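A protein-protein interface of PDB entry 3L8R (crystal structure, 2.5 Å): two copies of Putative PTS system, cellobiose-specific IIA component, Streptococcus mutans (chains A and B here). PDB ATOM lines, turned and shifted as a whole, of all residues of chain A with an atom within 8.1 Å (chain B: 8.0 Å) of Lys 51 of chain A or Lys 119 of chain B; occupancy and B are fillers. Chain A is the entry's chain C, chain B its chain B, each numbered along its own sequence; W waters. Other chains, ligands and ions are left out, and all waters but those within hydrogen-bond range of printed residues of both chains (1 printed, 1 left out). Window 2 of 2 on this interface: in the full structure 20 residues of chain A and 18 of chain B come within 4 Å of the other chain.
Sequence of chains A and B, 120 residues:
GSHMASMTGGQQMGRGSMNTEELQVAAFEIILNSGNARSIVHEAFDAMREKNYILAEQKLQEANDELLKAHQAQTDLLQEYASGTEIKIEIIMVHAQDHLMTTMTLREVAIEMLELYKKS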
ATOM      1  N   ALA A  44     -23.245 -25.821   6.766  1.00  0.00           N
ATOM      2  CA  ALA A  44     -22.029 -25.731   7.543  1.00  0.00           C
ATOM      3  C   ALA A  44     -22.332 -25.583   9.039  1.00  0.00           C
ATOM      4  O   ALA A  44     -21.539 -26.023   9.899  1.00  0.00           O
ATOM      5  CB  ALA A  44     -21.155 -24.638   7.023  1.00  0.00           C
ATOM      6  N   PHE A  45     -23.478 -24.989   9.356  1.00  0.00           N
ATOM      7  CA  PHE A  45     -23.874 -24.907  10.739  1.00  0.00           C
ATOM      8  C   PHE A  45     -24.221 -26.291  11.216  1.00  0.00           C
ATOM      9  O   PHE A  45     -23.806 -26.692  12.308  1.00  0.00           O
ATOM     10  CB  PHE A  45     -25.054 -23.947  10.962  1.00  0.00           C
ATOM     11  CG  PHE A  45     -24.638 -22.518  11.166  1.00  0.00           C
ATOM     12  CD1 PHE A  45     -25.257 -21.497  10.463  1.00  0.00           C
ATOM     13  CD2 PHE A  45     -23.580 -22.202  12.042  1.00  0.00           C
ATOM     14  CE1 PHE A  45     -24.867 -20.205  10.633  1.00  0.00           C
ATOM     15  CE2 PHE A  45     -23.168 -20.899  12.230  1.00  0.00           C
ATOM     16  CZ  PHE A  45     -23.803 -19.892  11.528  1.00  0.00           C
ATOM     17  N   ASP A  46     -24.985 -27.018  10.400  1.00  0.00           N
ATOM     18  CA  ASP A  46     -25.419 -28.362  10.740  1.00  0.00           C
ATOM     19  C   ASP A  46     -24.173 -29.207  11.003  1.00  0.00           C
ATOM     20  O   ASP A  46     -24.124 -29.921  11.999  1.00  0.00           O
ATOM     21  CB  ASP A  46     -26.282 -28.965   9.628  1.00  0.00           C
ATOM     22  CG  ASP A  46     -27.617 -28.198   9.408  1.00  0.00           C
ATOM     23  OD1 ASP A  46     -28.249 -27.734  10.401  1.00  0.00           O
ATOM     24  OD2 ASP A  46     -28.043 -28.084   8.224  1.00  0.00           O
ATOM     25  N   ALA A  47     -23.149 -29.073  10.155  1.00  0.00           N
ATOM     26  CA  ALA A  47     -21.876 -29.780  10.356  1.00  0.00           C
ATOM     27  C   ALA A  47     -21.137 -29.411  11.650  1.00  0.00           C
ATOM     28  O   ALA A  47     -20.582 -30.283  12.293  1.00  0.00           O
ATOM     29  CB  ALA A  47     -20.953 -29.634   9.149  1.00  0.00           C
ATOM     30  N   MET A  48     -21.124 -28.138  12.040  1.00  0.00           N
ATOM     31  CA  MET A  48     -20.513 -27.775  13.321  1.00  0.00           C
ATOM     32  C   MET A  48     -21.256 -28.444  14.482  1.00  0.00           C
ATOM     33  O   MET A  48     -20.690 -28.617  15.564  1.00  0.00           O
ATOM     34  CB  MET A  48     -20.500 -26.272  13.539  1.00  0.00           C
ATOM     35  CG  MET A  48     -19.772 -25.466  12.500  1.00  0.00           C
ATOM     36  SD  MET A  48     -20.092 -23.682  12.754  1.00  0.00           S
ATOM     37  CE  MET A  48     -19.946 -23.193  11.042  1.00  0.00           C
ATOM     38  N   ARG A  49     -22.519 -28.807  14.251  1.00  0.00           N
ATOM     39  CA  ARG A  49     -23.312 -29.524  15.259  1.00  0.00           C
ATOM     40  C   ARG A  49     -22.968 -31.018  15.319  1.00  0.00           C
ATOM     41  O   ARG A  49     -23.176 -31.668  16.340  1.00  0.00           O
ATOM     42  CB  ARG A  49     -24.820 -29.372  15.003  1.00  0.00           C
ATOM     43  CG  ARG A  49     -25.443 -28.190  15.689  1.00  0.00           C
ATOM     44  CD  ARG A  49     -25.595 -27.032  14.753  1.00  0.00           C
ATOM     45  NE  ARG A  49     -26.952 -26.826  14.218  1.00  0.00           N
ATOM     46  CZ  ARG A  49     -28.011 -26.586  14.985  1.00  0.00           C
ATOM     47  NH1 ARG A  49     -27.873 -26.603  16.285  1.00  0.00           N
ATOM     48  NH2 ARG A  49     -29.214 -26.357  14.469  1.00  0.00           N
ATOM     49  N   GLU A  50     -22.473 -31.565  14.216  1.00  0.00           N
ATOM     50  CA  GLU A  50     -22.120 -32.967  14.196  1.00  0.00           C
ATOM     51  C   GLU A  50     -20.683 -33.118  14.649  1.00  0.00           C
ATOM     52  O   GLU A  50     -20.204 -34.243  14.815  1.00  0.00           O
ATOM     53  CB  GLU A  50     -22.320 -33.579  12.799  1.00  0.00           C
ATOM     54  CG  GLU A  50     -23.739 -33.481  12.218  1.00  0.00           C
ATOM     55  CD  GLU A  50     -24.882 -33.745  13.212  1.00  0.00           C
ATOM     56  OE1 GLU A  50     -24.659 -34.230  14.354  1.00  0.00           O
ATOM     57  OE2 GLU A  50     -26.033 -33.447  12.822  1.00  0.00           O
ATOM     58  N   LYS A  51     -20.028 -31.971  14.876  1.00  0.00           N
ATOM     59  CA  LYS A  51     -18.596 -31.875  15.162  1.00  0.00           C
ATOM     60  C   LYS A  51     -17.830 -32.261  13.906  1.00  0.00           C
ATOM     61  O   LYS A  51     -16.733 -32.789  13.976  1.00  0.00           O
ATOM     62  CB  LYS A  51     -18.188 -32.739  16.376  1.00  0.00           C
ATOM     63  CG  LYS A  51     -17.951 -31.979  17.680  1.00  0.00           C
ATOM     64  CD  LYS A  51     -19.029 -30.893  17.956  1.00  0.00           C
ATOM     65  CE  LYS A  51     -20.244 -31.405  18.779  1.00  0.00           C
ATOM     66  NZ  LYS A  51     -21.307 -30.341  18.828  1.00  0.00           N
ATOM     67  N   ASN A  52     -18.442 -32.006  12.758  1.00  0.00           N
ATOM     68  CA  ASN A  52     -17.846 -32.231  11.455  1.00  0.00           C
ATOM     69  C   ASN A  52     -17.117 -30.992  10.974  1.00  0.00           C
ATOM     70  O   ASN A  52     -17.524 -30.369   9.999  1.00  0.00           O
ATOM     71  CB  ASN A  52     -18.955 -32.505  10.455  1.00  0.00           C
ATOM     72  CG  ASN A  52     -19.099 -33.947  10.116  1.00  0.00           C
ATOM     73  OD1 ASN A  52     -20.003 -34.632  10.624  1.00  0.00           O
ATOM     74  ND2 ASN A  52     -18.234 -34.426   9.214  1.00  0.00           N
ATOM     75  N   TYR A  53     -16.021 -30.645  11.627  1.00  0.00           N
ATOM     76  CA  TYR A  53     -15.413 -29.332  11.422  1.00  0.00           C
ATOM     77  C   TYR A  53     -14.721 -29.121  10.097  1.00  0.00           C
ATOM     78  O   TYR A  53     -14.161 -28.061   9.856  1.00  0.00           O
ATOM     79  CB  TYR A  53     -14.437 -29.046  12.533  1.00  0.00           C
ATOM     80  CG  TYR A  53     -15.117 -29.004  13.859  1.00  0.00           C
ATOM     81  CD1 TYR A  53     -16.422 -28.509  13.973  1.00  0.00           C
ATOM     82  CD2 TYR A  53     -14.455 -29.439  15.016  1.00  0.00           C
ATOM     83  CE1 TYR A  53     -17.051 -28.455  15.206  1.00  0.00           C
ATOM     84  CE2 TYR A  53     -15.088 -29.392  16.266  1.00  0.00           C
ATOM     85  CZ  TYR A  53     -16.381 -28.896  16.349  1.00  0.00           C
ATOM     86  OH  TYR A  53     -17.003 -28.858  17.571  1.00  0.00           O
ATOM     87  N   ILE A  54     -14.773 -30.120   9.238  1.00  0.00           N
ATOM     88  CA  ILE A  54     -13.979 -30.157   8.033  1.00  0.00           C
ATOM     89  C   ILE A  54     -15.000 -30.103   6.915  1.00  0.00           C
ATOM     90  O   ILE A  54     -14.800 -29.470   5.882  1.00  0.00           O
ATOM     91  CB  ILE A  54     -13.185 -31.487   8.025  1.00  0.00           C
ATOM     92  CG1 ILE A  54     -11.883 -31.431   7.230  1.00  0.00           C
ATOM     93  CG2 ILE A  54     -14.065 -32.652   7.522  1.00  0.00           C
ATOM     94  CD1 ILE A  54     -10.812 -32.470   7.799  1.00  0.00           C
ATOM     95  N   LEU A  55     -16.113 -30.784   7.136  1.00  0.00           N
ATOM     96  CA  LEU A  55     -17.277 -30.639   6.300  1.00  0.00           C
ATOM     97  C   LEU A  55     -17.664 -29.160   6.339  1.00  0.00           C
ATOM     98  O   LEU A  55     -17.563 -28.465   5.326  1.00  0.00           O
ATOM     99  CB  LEU A  55     -18.403 -31.498   6.858  1.00  0.00           C
ATOM    100  CG  LEU A  55     -19.359 -32.202   5.898  1.00  0.00           C
ATOM    101  CD1 LEU A  55     -20.752 -32.092   6.506  1.00  0.00           C
ATOM    102  CD2 LEU A  55     -19.283 -31.638   4.462  1.00  0.00           C
ATOM    103  N   ALA A  56     -18.025 -28.684   7.529  1.00  0.00           N
ATOM    104  CA  ALA A  56     -18.325 -27.280   7.768  1.00  0.00           C
ATOM    105  C   ALA A  56     -17.355 -26.338   7.068  1.00  0.00           C
ATOM    106  O   ALA A  56     -17.815 -25.436   6.367  1.00  0.00           O
ATOM    107  CB  ALA A  56     -18.394 -26.982   9.261  1.00  0.00           C
ATOM    108  N   LEU A 116     -14.646 -20.708  16.947  1.00  0.00           N
ATOM    109  CA  LEU A 116     -15.131 -20.924  18.327  1.00  0.00           C
ATOM    110  C   LEU A 116     -15.377 -22.413  18.568  1.00  0.00           C
ATOM    111  O   LEU A 116     -14.695 -23.003  19.368  1.00  0.00           O
ATOM    112  CB  LEU A 116     -16.373 -20.085  18.657  1.00  0.00           C
ATOM    113  CG  LEU A 116     -16.410 -19.274  19.963  1.00  0.00           C
ATOM    114  CD1 LEU A 116     -17.828 -19.082  20.484  1.00  0.00           C
ATOM    115  CD2 LEU A 116     -15.549 -19.850  21.095  1.00  0.00           C
ATOM    116  N   TYR A 117     -16.302 -23.028  17.832  1.00  0.00           N
ATOM    117  CA  TYR A 117     -16.535 -24.492  17.896  1.00  0.00           C
ATOM    118  C   TYR A 117     -15.237 -25.281  18.081  1.00  0.00           C
ATOM    119  O   TYR A 117     -15.163 -26.183  18.925  1.00  0.00           O
ATOM    120  CB  TYR A 117     -17.263 -25.002  16.634  1.00  0.00           C
ATOM    121  CG  TYR A 117     -18.759 -25.184  16.809  1.00  0.00           C
ATOM    122  CD1 TYR A 117     -19.278 -26.338  17.429  1.00  0.00           C
ATOM    123  CD2 TYR A 117     -19.666 -24.218  16.360  1.00  0.00           C
ATOM    124  CE1 TYR A 117     -20.632 -26.516  17.602  1.00  0.00           C
ATOM    125  CE2 TYR A 117     -21.036 -24.404  16.526  1.00  0.00           C
ATOM    126  CZ  TYR A 117     -21.497 -25.552  17.147  1.00  0.00           C
ATOM    127  OH  TYR A 117     -22.830 -25.740  17.315  1.00  0.00           O
ATOM    128  N   LYS A 118     -14.218 -24.943  17.286  1.00  0.00           N
ATOM    129  CA  LYS A 118     -12.909 -25.620  17.348  1.00  0.00           C
ATOM    130  C   LYS A 118     -12.119 -25.199  18.593  1.00  0.00           C
ATOM    131  O   LYS A 118     -11.011 -24.703  18.476  1.00  0.00           O
ATOM    132  CB  LYS A 118     -12.094 -25.368  16.053  1.00  0.00           C
ATOM    133  CG  LYS A 118     -12.703 -25.983  14.803  1.00  0.00           C
ATOM    134  CD  LYS A 118     -11.700 -26.068  13.662  1.00  0.00           C
ATOM    135  CE  LYS A 118     -11.520 -24.767  12.891  1.00  0.00           C
ATOM    136  NZ  LYS A 118     -10.774 -25.032  11.631  1.00  0.00           N
ATOM    137  N   LYS A 119     -12.707 -25.390  19.772  1.00  0.00           N
ATOM    138  CA  LYS A 119     -12.113 -25.006  21.059  1.00  0.00           C
ATOM    139  C   LYS A 119     -12.974 -25.597  22.166  1.00  0.00           C
ATOM    140  O   LYS A 119     -14.206 -25.571  22.074  1.00  0.00           O
ATOM    141  CB  LYS A 119     -12.026 -23.465  21.221  1.00  0.00           C
ATOM    142  CG  LYS A 119     -10.773 -22.867  20.591  1.00  0.00           C
ATOM    143  CD  LYS A 119     -10.925 -21.425  20.155  1.00  0.00           C
ATOM    144  CE  LYS A 119      -9.920 -21.118  19.052  1.00  0.00           C
ATOM    145  NZ  LYS A 119      -9.978 -19.704  18.642  1.00  0.00           N
ATOM    146  N   TYR B  53     -30.910 -21.278  29.472  1.00  0.00           N
ATOM    147  CA  TYR B  53     -31.243 -21.673  28.115  1.00  0.00           C
ATOM    148  C   TYR B  53     -32.695 -21.837  27.842  1.00  0.00           C
ATOM    149  O   TYR B  53     -33.116 -21.641  26.705  1.00  0.00           O
ATOM    150  CB  TYR B  53     -30.516 -22.929  27.679  1.00  0.00           C
ATOM    151  CG  TYR B  53     -29.055 -22.864  27.993  1.00  0.00           C
ATOM    152  CD1 TYR B  53     -28.339 -21.675  27.813  1.00  0.00           C
ATOM    153  CD2 TYR B  53     -28.384 -23.974  28.496  1.00  0.00           C
ATOM    154  CE1 TYR B  53     -26.981 -21.601  28.122  1.00  0.00           C
ATOM    155  CE2 TYR B  53     -27.025 -23.905  28.811  1.00  0.00           C
ATOM    156  CZ  TYR B  53     -26.338 -22.724  28.620  1.00  0.00           C
ATOM    157  OH  TYR B  53     -25.006 -22.656  28.932  1.00  0.00           O
ATOM    158  N   MET B 113     -26.041 -19.829  18.051  1.00  0.00           N
ATOM    159  CA  MET B 113     -25.275 -19.554  19.241  1.00  0.00           C
ATOM    160  C   MET B 113     -25.868 -20.173  20.501  1.00  0.00           C
ATOM    161  O   MET B 113     -25.170 -20.432  21.465  1.00  0.00           O
ATOM    162  CB  MET B 113     -25.035 -18.069  19.393  1.00  0.00           C
ATOM    163  CG  MET B 113     -23.780 -17.631  18.664  1.00  0.00           C
ATOM    164  SD  MET B 113     -23.496 -15.894  18.936  1.00  0.00           S
ATOM    165  CE  MET B 113     -22.706 -15.929  20.555  1.00  0.00           C
ATOM    166  N   LEU B 114     -27.159 -20.427  20.504  1.00  0.00           N
ATOM    167  CA  LEU B 114     -27.737 -21.075  21.651  1.00  0.00           C
ATOM    168  C   LEU B 114     -27.069 -22.438  21.714  1.00  0.00           C
ATOM    169  O   LEU B 114     -26.703 -22.963  22.788  1.00  0.00           O
ATOM    170  CB  LEU B 114     -29.234 -21.253  21.437  1.00  0.00           C
ATOM    171  CG  LEU B 114     -30.197 -21.029  22.590  1.00  0.00           C
ATOM    172  CD1 LEU B 114     -31.508 -21.645  22.180  1.00  0.00           C
ATOM    173  CD2 LEU B 114     -29.655 -21.606  23.910  1.00  0.00           C
ATOM    174  N   GLU B 115     -26.895 -23.012  20.536  1.00  0.00           N
ATOM    175  CA  GLU B 115     -26.397 -24.355  20.471  1.00  0.00           C
ATOM    176  C   GLU B 115     -24.930 -24.517  20.978  1.00  0.00           C
ATOM    177  O   GLU B 115     -24.602 -25.477  21.658  1.00  0.00           O
ATOM    178  CB  GLU B 115     -26.646 -24.897  19.073  1.00  0.00           C
ATOM    179  CG  GLU B 115     -27.034 -26.333  19.095  1.00  0.00           C
ATOM    180  CD  GLU B 115     -28.500 -26.558  19.393  1.00  0.00           C
ATOM    181  OE1 GLU B 115     -29.268 -25.566  19.568  1.00  0.00           O
ATOM    182  OE2 GLU B 115     -28.863 -27.760  19.434  1.00  0.00           O
ATOM    183  N   LEU B 116     -24.043 -23.583  20.676  1.00  0.00           N
ATOM    184  CA  LEU B 116     -22.743 -23.612  21.338  1.00  0.00           C
ATOM    185  C   LEU B 116     -22.986 -23.408  22.821  1.00  0.00           C
ATOM    186  O   LEU B 116     -22.612 -24.233  23.641  1.00  0.00           O
ATOM    187  CB  LEU B 116     -21.839 -22.487  20.852  1.00  0.00           C
ATOM    188  CG  LEU B 116     -20.802 -22.789  19.802  1.00  0.00           C
ATOM    189  CD1 LEU B 116     -20.185 -21.484  19.439  1.00  0.00           C
ATOM    190  CD2 LEU B 116     -19.759 -23.727  20.337  1.00  0.00           C
ATOM    191  N   TYR B 117     -23.618 -22.306  23.179  1.00  0.00           N
ATOM    192  CA  TYR B 117     -23.873 -22.072  24.587  1.00  0.00           C
ATOM    193  C   TYR B 117     -24.187 -23.372  25.358  1.00  0.00           C
ATOM    194  O   TYR B 117     -23.488 -23.687  26.331  1.00  0.00           O
ATOM    195  CB  TYR B 117     -24.956 -21.005  24.805  1.00  0.00           C
ATOM    196  CG  TYR B 117     -24.385 -19.683  25.245  1.00  0.00           C
ATOM    197  CD1 TYR B 117     -23.613 -19.587  26.407  1.00  0.00           C
ATOM    198  CD2 TYR B 117     -24.615 -18.528  24.522  1.00  0.00           C
ATOM    199  CE1 TYR B 117     -23.109 -18.377  26.834  1.00  0.00           C
ATOM    200  CE2 TYR B 117     -24.115 -17.296  24.955  1.00  0.00           C
ATOM    201  CZ  TYR B 117     -23.356 -17.239  26.097  1.00  0.00           C
ATOM    202  OH  TYR B 117     -22.833 -16.040  26.498  1.00  0.00           O
ATOM    203  N   LYS B 118     -25.200 -24.121  24.904  1.00  0.00           N
ATOM    204  CA  LYS B 118     -25.661 -25.352  25.561  1.00  0.00           C
ATOM    205  C   LYS B 118     -24.573 -26.429  25.720  1.00  0.00           C
ATOM    206  O   LYS B 118     -24.802 -27.463  26.366  1.00  0.00           O
ATOM    207  CB  LYS B 118     -26.894 -25.925  24.849  1.00  0.00           C
ATOM    208  CG  LYS B 118     -28.245 -25.394  25.346  1.00  0.00           C
ATOM    209  CD  LYS B 118     -29.383 -25.806  24.405  1.00  0.00           C
ATOM    210  CE  LYS B 118     -30.738 -25.827  25.091  1.00  0.00           C
ATOM    211  NZ  LYS B 118     -31.690 -24.763  24.622  1.00  0.00           N
ATOM    212  N   LYS B 119     -23.395 -26.196  25.142  1.00  0.00           N
ATOM    213  CA  LYS B 119     -22.210 -26.980  25.508  1.00  0.00           C
ATOM    214  C   LYS B 119     -21.046 -26.058  25.865  1.00  0.00           C
ATOM    215  O   LYS B 119     -19.876 -26.445  25.792  1.00  0.00           O
ATOM    216  CB  LYS B 119     -21.825 -27.971  24.404  1.00  0.00           C
ATOM    217  CG  LYS B 119     -21.937 -27.406  23.003  1.00  0.00           C
ATOM    218  CD  LYS B 119     -20.910 -28.009  22.018  1.00  0.00           C
ATOM    219  CE  LYS B 119     -19.452 -27.493  22.235  1.00  0.00           C
ATOM    220  NZ  LYS B 119     -18.453 -28.384  21.558  1.00  0.00           N
HETATM  221  O   HOH W   1     -15.170 -28.405  21.968  1.00  0.00           O
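Leu 116 of chain A touches its own counterpart, Leu 116 of chain B.
Tyr 117 of chain A touches Leu 116 of chain B, but with the chains exchanged Leu 116 of chain A does not touch Tyr 117 of chain B (7.2 Å).
Of the 4 pairs that touch across the chains among the printed residues, 1 has its exchanged pair printed and touching as well.
Hydrophobic or aromatic side chains of chain B within 4 Å of the printed part of chain A: Leu 116.
Hydrophobic or aromatic side chains of chain A that line the printed part of chain B: Leu 116 and Tyr 117.
Lys 51 of chain A touches Lys 119 of chain B (NZ to CD, 3.97 Å).
CD1 of Leu 116 of chain A touches CD1 of Leu 116 of chain B, 3.5 Å away.
Tyr 117 of chain A touches Leu 116 of chain B (CE2 to CG, 3.7 Å).
The side-chain carboxylate (OE2) of Glu 115 of chain B lies within salt-bridge range of the guanidinium group (NH1) of Arg 49 of chain A (3.5 Å).
Water W1 lies within hydrogen-bond range of O of Lys 119 of chain A and NZ of Lys 119 of chain B.
The backbone carbonyl oxygen (O) of Arg 49 of chain A lies within hydrogen-bond range of the side-chain amino group (NZ) of Lys 51 of chain A, at 3.4 Å.
Lys 51 of chain A touches one residue of chain B.
Lys 119 of chain B touches just one residue of chain A: Lys 51.
Printed residues of chain B within 4 Å of Tyr 117 of chain A: Leu 116 (3.7 Å).
Printed residues of chain B within 4 Å of Leu 116 of chain A: Leu 116 (3.5 Å).
Ile 54 of chain A touches none of the printed residues of chain B.
The nearest residue of chain B that does not touch Lys 51 of chain A is Glu 115 of chain B (6.5 Å).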
